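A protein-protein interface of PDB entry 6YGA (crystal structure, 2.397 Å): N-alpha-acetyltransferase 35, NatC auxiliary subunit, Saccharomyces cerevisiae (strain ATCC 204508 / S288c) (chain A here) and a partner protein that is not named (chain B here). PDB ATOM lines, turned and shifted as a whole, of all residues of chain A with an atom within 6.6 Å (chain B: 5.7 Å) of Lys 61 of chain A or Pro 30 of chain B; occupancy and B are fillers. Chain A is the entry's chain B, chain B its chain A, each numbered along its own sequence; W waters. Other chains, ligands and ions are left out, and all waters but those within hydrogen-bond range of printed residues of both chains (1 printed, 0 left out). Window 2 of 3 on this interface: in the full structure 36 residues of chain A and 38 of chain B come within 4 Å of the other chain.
Printed residues of chain A that touch a printed residue of chain B: Ser 54, Glu 56, Lys 61 and Leu 62.
Hydrophobic or aromatic side chains of chain A that line the printed part of chain B: Leu 62.
Along chain A the printed residues that touch a printed residue of chain B span positions 54 to 62.
Hydrophobic or aromatic side chains of chain B that line the printed part of chain A: Pro 30.
OG of Ser 32 of chain B is in hydrogen-bond range of OG of Ser 54 of chain A (2.8 Å).
O of Ser 28 of chain B sits at hydrogen-bond distance from NZ of Lys 61 of chain A.
NZ of Lys 61 of chain A sits at hydrogen-bond distance from O of Leu 27 of chain B.
The side-chain amide oxygen (OD1) of Asn 59 of chain A lies close to the backbone NH (N) of Lys 61 of chain A (3.2 Å).
Ser 60 of chain A touches none of the printed residues of chain B.
Of the printed residues of chain B, Lys 61 of chain A touches Asp 24, Leu 27, Ser 28 and Pro 30.
Of the printed residues of chain B, Leu 62 of chain A touches Pro 30, Tyr 31 and Ser 32.
Pro 286 of chain A touches none of the printed residues of chain B.
Of the printed residues of chain A, Asp 24 of chain B touches Lys 61 (3.996 Å).
Of the printed residues of chain A, Ser 28 of chain B touches Lys 61 (3.2 Å).
Pro 30 of chain B touches two residues of chain A.
Printed residues of chain A within 4 Å of Ser 32 of chain B: Ser 54 (2.8 Å), Glu 56 (3.5 Å) and Leu 62 (3.9 Å).
The nearest residue of chain A that does not touch Pro 30 of chain B is Asn 59 of chain A (4.2 Å).
Water W1 lies within hydrogen-bond range of O of Ser 54 of chain A (2.5 Å), OG of Ser 32 of chain B (3.1 Å) and O of Thr 52 of chain A (3.1 Å).
OE2 of Glu 56 of chain A touches CA of Ser 32 of chain B, at 3.5 Å.
O of Asp 24 of chain B touches NZ of Lys 61 of chain A, at 3.996 Å.
CG of Pro 30 of chain B touches CB of Lys 61 of chain A, at 3.5 Å.
Leu 62 of chain A touches Pro 30 of chain B (CG to CG, 3.6 Å).
C of Tyr 31 of chain B touches CD1 of Leu 62 of chain A (3.9 Å).
Ser 32 of chain B touches Leu 62 of chain A (N to CD1, 3.9 Å).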
ATOM      1  N   THR A  52      16.496  19.540  -4.011  1.00  0.00           N
ATOM      2  CA  THR A  52      16.269  19.675  -5.446  1.00  0.00           C
ATOM      3  C   THR A  52      14.912  19.135  -5.864  1.00  0.00           C
ATOM      4  O   THR A  52      14.454  19.426  -6.976  1.00  0.00           O
ATOM      5  CB  THR A  52      17.377  18.970  -6.238  1.00  0.00           C
ATOM      6  OG1 THR A  52      17.418  17.583  -5.878  1.00  0.00           O
ATOM      7  CG2 THR A  52      18.724  19.615  -5.951  1.00  0.00           C
ATOM      8  N   SER A  54      11.962  19.774  -4.218  1.00  0.00           N
ATOM      9  CA  SER A  54      11.076  20.509  -3.326  1.00  0.00           C
ATOM     10  C   SER A  54      10.016  21.260  -4.118  1.00  0.00           C
ATOM     11  O   SER A  54      10.258  21.718  -5.238  1.00  0.00           O
ATOM     12  CB  SER A  54      11.857  21.502  -2.455  1.00  0.00           C
ATOM     13  OG  SER A  54      12.547  22.460  -3.248  1.00  0.00           O
ATOM     14  N   GLU A  56       7.249  24.551  -4.374  1.00  0.00           N
ATOM     15  CA  GLU A  56       7.396  25.989  -4.184  1.00  0.00           C
ATOM     16  C   GLU A  56       6.030  26.656  -4.258  1.00  0.00           C
ATOM     17  O   GLU A  56       5.292  26.460  -5.230  1.00  0.00           O
ATOM     18  CB  GLU A  56       8.339  26.593  -5.229  1.00  0.00           C
ATOM     19  CG  GLU A  56       8.900  27.939  -4.814  1.00  0.00           C
ATOM     20  CD  GLU A  56      10.144  28.321  -5.584  1.00  0.00           C
ATOM     21  OE1 GLU A  56      10.028  28.655  -6.781  1.00  0.00           O
ATOM     22  OE2 GLU A  56      11.242  28.275  -4.992  1.00  0.00           O
ATOM     23  N   ASN A  58       3.111  29.548  -4.606  1.00  0.00           N
ATOM     24  CA  ASN A  58       2.864  30.654  -5.531  1.00  0.00           C
ATOM     25  C   ASN A  58       3.625  30.481  -6.847  1.00  0.00           C
ATOM     26  O   ASN A  58       3.931  31.457  -7.537  1.00  0.00           O
ATOM     27  CB  ASN A  58       3.189  32.001  -4.875  1.00  0.00           C
ATOM     28  CG  ASN A  58       2.262  32.314  -3.716  1.00  0.00           C
ATOM     29  OD1 ASN A  58       1.061  32.061  -3.786  1.00  0.00           O
ATOM     30  ND2 ASN A  58       2.819  32.848  -2.633  1.00  0.00           N
ATOM     31  N   ASN A  59       3.942  29.233  -7.190  1.00  0.00           N
ATOM     32  CA  ASN A  59       4.481  28.860  -8.494  1.00  0.00           C
ATOM     33  C   ASN A  59       3.462  27.922  -9.125  1.00  0.00           C
ATOM     34  O   ASN A  59       3.270  26.801  -8.644  1.00  0.00           O
ATOM     35  CB  ASN A  59       5.852  28.197  -8.365  1.00  0.00           C
ATOM     36  CG  ASN A  59       6.534  27.994  -9.706  1.00  0.00           C
ATOM     37  OD1 ASN A  59       5.889  27.692 -10.710  1.00  0.00           O
ATOM     38  ND2 ASN A  59       7.850  28.166  -9.728  1.00  0.00           N
ATOM     39  N   SER A  60       2.806  28.391 -10.188  1.00  0.00           N
ATOM     40  CA  SER A  60       1.700  27.645 -10.784  1.00  0.00           C
ATOM     41  C   SER A  60       2.095  26.209 -11.104  1.00  0.00           C
ATOM     42  O   SER A  60       1.316  25.276 -10.875  1.00  0.00           O
ATOM     43  CB  SER A  60       1.215  28.358 -12.047  1.00  0.00           C
ATOM     44  OG  SER A  60       1.031  29.743 -11.809  1.00  0.00           O
ATOM     45  N   LYS A  61       3.308  26.011 -11.619  1.00  0.00           N
ATOM     46  CA  LYS A  61       3.742  24.691 -12.056  1.00  0.00           C
ATOM     47  C   LYS A  61       4.257  23.821 -10.913  1.00  0.00           C
ATOM     48  O   LYS A  61       4.423  22.613 -11.106  1.00  0.00           O
ATOM     49  CB  LYS A  61       4.818  24.838 -13.137  1.00  0.00           C
ATOM     50  CG  LYS A  61       4.520  25.927 -14.162  1.00  0.00           C
ATOM     51  CD  LYS A  61       5.225  25.672 -15.492  1.00  0.00           C
ATOM     52  CE  LYS A  61       6.730  25.882 -15.399  1.00  0.00           C
ATOM     53  NZ  LYS A  61       7.421  25.495 -16.666  1.00  0.00           N
ATOM     54  N   LEU A  62       4.492  24.395  -9.731  1.00  0.00           N
ATOM     55  CA  LEU A  62       4.996  23.649  -8.582  1.00  0.00           C
ATOM     56  C   LEU A  62       4.077  23.717  -7.365  1.00  0.00           C
ATOM     57  O   LEU A  62       4.450  23.216  -6.297  1.00  0.00           O
ATOM     58  CB  LEU A  62       6.389  24.151  -8.190  1.00  0.00           C
ATOM     59  CG  LEU A  62       7.577  23.705  -9.043  1.00  0.00           C
ATOM     60  CD1 LEU A  62       8.832  24.475  -8.656  1.00  0.00           C
ATOM     61  CD2 LEU A  62       7.803  22.209  -8.902  1.00  0.00           C
ATOM     62  N   ASP A  63       2.893  24.317  -7.486  1.00  0.00           N
ATOM     63  CA  ASP A  63       1.977  24.490  -6.359  1.00  0.00           C
ATOM     64  C   ASP A  63       0.621  23.907  -6.741  1.00  0.00           C
ATOM     65  O   ASP A  63      -0.110  24.502  -7.541  1.00  0.00           O
ATOM     66  CB  ASP A  63       1.851  25.968  -5.974  1.00  0.00           C
ATOM     67  CG  ASP A  63       1.200  26.178  -4.609  1.00  0.00           C
ATOM     68  OD1 ASP A  63       0.480  25.278  -4.132  1.00  0.00           O
ATOM     69  OD2 ASP A  63       1.406  27.258  -4.013  1.00  0.00           O
ATOM     70  N   SER A  64       0.282  22.752  -6.159  1.00  0.00           N
ATOM     71  CA  SER A  64      -1.008  22.121  -6.415  1.00  0.00           C
ATOM     72  C   SER A  64      -2.163  22.850  -5.734  1.00  0.00           C
ATOM     73  O   SER A  64      -3.325  22.599  -6.073  1.00  0.00           O
ATOM     74  CB  SER A  64      -0.974  20.655  -5.971  1.00  0.00           C
ATOM     75  OG  SER A  64      -0.464  20.525  -4.655  1.00  0.00           O
ATOM     76  N   PRO A 286       4.371  17.968  -7.744  1.00  0.00           N
ATOM     77  CA  PRO A 286       3.794  19.092  -8.500  1.00  0.00           C
ATOM     78  C   PRO A 286       2.513  18.673  -9.197  1.00  0.00           C
ATOM     79  O   PRO A 286       2.306  17.479  -9.466  1.00  0.00           O
ATOM     80  CB  PRO A 286       4.893  19.438  -9.518  1.00  0.00           C
ATOM     81  CG  PRO A 286       6.147  18.862  -8.945  1.00  0.00           C
ATOM     82  CD  PRO A 286       5.722  17.623  -8.218  1.00  0.00           C
ATOM     83  N   PRO A 287       1.624  19.618  -9.498  1.00  0.00           N
ATOM     84  CA  PRO A 287       0.381  19.264 -10.190  1.00  0.00           C
ATOM     85  C   PRO A 287       0.636  18.883 -11.639  1.00  0.00           C
ATOM     86  O   PRO A 287       1.532  19.414 -12.298  1.00  0.00           O
ATOM     87  CB  PRO A 287      -0.450  20.546 -10.094  1.00  0.00           C
ATOM     88  CG  PRO A 287       0.561  21.630 -10.017  1.00  0.00           C
ATOM     89  CD  PRO A 287       1.705  21.062  -9.217  1.00  0.00           C
ATOM     90  N   ASP B  24      13.698  28.891 -16.485  1.00  0.00           N
ATOM     91  CA  ASP B  24      12.310  28.487 -16.259  1.00  0.00           C
ATOM     92  C   ASP B  24      11.469  28.578 -17.526  1.00  0.00           C
ATOM     93  O   ASP B  24      10.518  27.804 -17.689  1.00  0.00           O
ATOM     94  CB  ASP B  24      11.680  29.338 -15.155  1.00  0.00           C
ATOM     95  CG  ASP B  24      12.114  28.910 -13.768  1.00  0.00           C
ATOM     96  OD1 ASP B  24      12.580  27.761 -13.616  1.00  0.00           O
ATOM     97  OD2 ASP B  24      11.981  29.720 -12.829  1.00  0.00           O
ATOM     98  N   LEU B  27      11.798  25.213 -19.487  1.00  0.00           N
ATOM     99  CA  LEU B  27      11.402  23.975 -18.830  1.00  0.00           C
ATOM    100  C   LEU B  27       9.898  23.750 -18.910  1.00  0.00           C
ATOM    101  O   LEU B  27       9.104  24.665 -18.679  1.00  0.00           O
ATOM    102  CB  LEU B  27      11.829  23.993 -17.365  1.00  0.00           C
ATOM    103  CG  LEU B  27      13.316  24.176 -17.069  1.00  0.00           C
ATOM    104  CD1 LEU B  27      13.572  24.023 -15.581  1.00  0.00           C
ATOM    105  CD2 LEU B  27      14.164  23.204 -17.878  1.00  0.00           C
ATOM    106  N   SER B  28       9.513  22.513 -19.231  1.00  0.00           N
ATOM    107  CA  SER B  28       8.130  22.099 -19.038  1.00  0.00           C
ATOM    108  C   SER B  28       7.799  21.993 -17.553  1.00  0.00           C
ATOM    109  O   SER B  28       6.704  22.372 -17.122  1.00  0.00           O
ATOM    110  CB  SER B  28       7.882  20.769 -19.748  1.00  0.00           C
ATOM    111  OG  SER B  28       7.960  20.911 -21.156  1.00  0.00           O
ATOM    112  N   GLU B  29       8.735  21.483 -16.756  1.00  0.00           N
ATOM    113  CA  GLU B  29       8.586  21.396 -15.315  1.00  0.00           C
ATOM    114  C   GLU B  29       9.696  22.197 -14.648  1.00  0.00           C
ATOM    115  O   GLU B  29      10.877  21.998 -14.970  1.00  0.00           O
ATOM    116  CB  GLU B  29       8.615  19.932 -14.842  1.00  0.00           C
ATOM    117  CG  GLU B  29       7.298  19.208 -15.069  1.00  0.00           C
ATOM    118  CD  GLU B  29       7.481  17.786 -15.543  1.00  0.00           C
ATOM    119  OE1 GLU B  29       8.537  17.189 -15.244  1.00  0.00           O
ATOM    120  OE2 GLU B  29       6.568  17.272 -16.223  1.00  0.00           O
ATOM    121  N   PRO B  30       9.369  23.107 -13.731  1.00  0.00           N
ATOM    122  CA  PRO B  30      10.364  24.088 -13.286  1.00  0.00           C
ATOM    123  C   PRO B  30      11.172  23.643 -12.080  1.00  0.00           C
ATOM    124  O   PRO B  30      11.001  22.535 -11.562  1.00  0.00           O
ATOM    125  CB  PRO B  30       9.500  25.307 -12.953  1.00  0.00           C
ATOM    126  CG  PRO B  30       8.267  24.692 -12.386  1.00  0.00           C
ATOM    127  CD  PRO B  30       8.048  23.378 -13.140  1.00  0.00           C
ATOM    128  N   TYR B  31      12.061  24.519 -11.629  1.00  0.00           N
ATOM    129  CA  TYR B  31      12.908  24.275 -10.474  1.00  0.00           C
ATOM    130  C   TYR B  31      12.569  25.262  -9.363  1.00  0.00           C
ATOM    131  O   TYR B  31      12.203  26.411  -9.623  1.00  0.00           O
ATOM    132  CB  TYR B  31      14.392  24.400 -10.838  1.00  0.00           C
ATOM    133  CG  TYR B  31      14.844  23.448 -11.921  1.00  0.00           C
ATOM    134  CD1 TYR B  31      14.250  22.202 -12.069  1.00  0.00           C
ATOM    135  CD2 TYR B  31      15.863  23.797 -12.800  1.00  0.00           C
ATOM    136  CE1 TYR B  31      14.656  21.330 -13.057  1.00  0.00           C
ATOM    137  CE2 TYR B  31      16.279  22.929 -13.792  1.00  0.00           C
ATOM    138  CZ  TYR B  31      15.669  21.698 -13.916  1.00  0.00           C
ATOM    139  OH  TYR B  31      16.070  20.825 -14.900  1.00  0.00           O
ATOM    140  N   SER B  32      12.690  24.801  -8.122  1.00  0.00           N
ATOM    141  CA  SER B  32      12.500  25.691  -6.991  1.00  0.00           C
ATOM    142  C   SER B  32      13.737  26.564  -6.800  1.00  0.00           C
ATOM    143  O   SER B  32      14.776  26.365  -7.433  1.00  0.00           O
ATOM    144  CB  SER B  32      12.203  24.898  -5.718  1.00  0.00           C
ATOM    145  OG  SER B  32      13.359  24.227  -5.246  1.00  0.00           O
HETATM  146  O   HOH W   1      12.300  21.669  -6.595  1.00  0.00           O
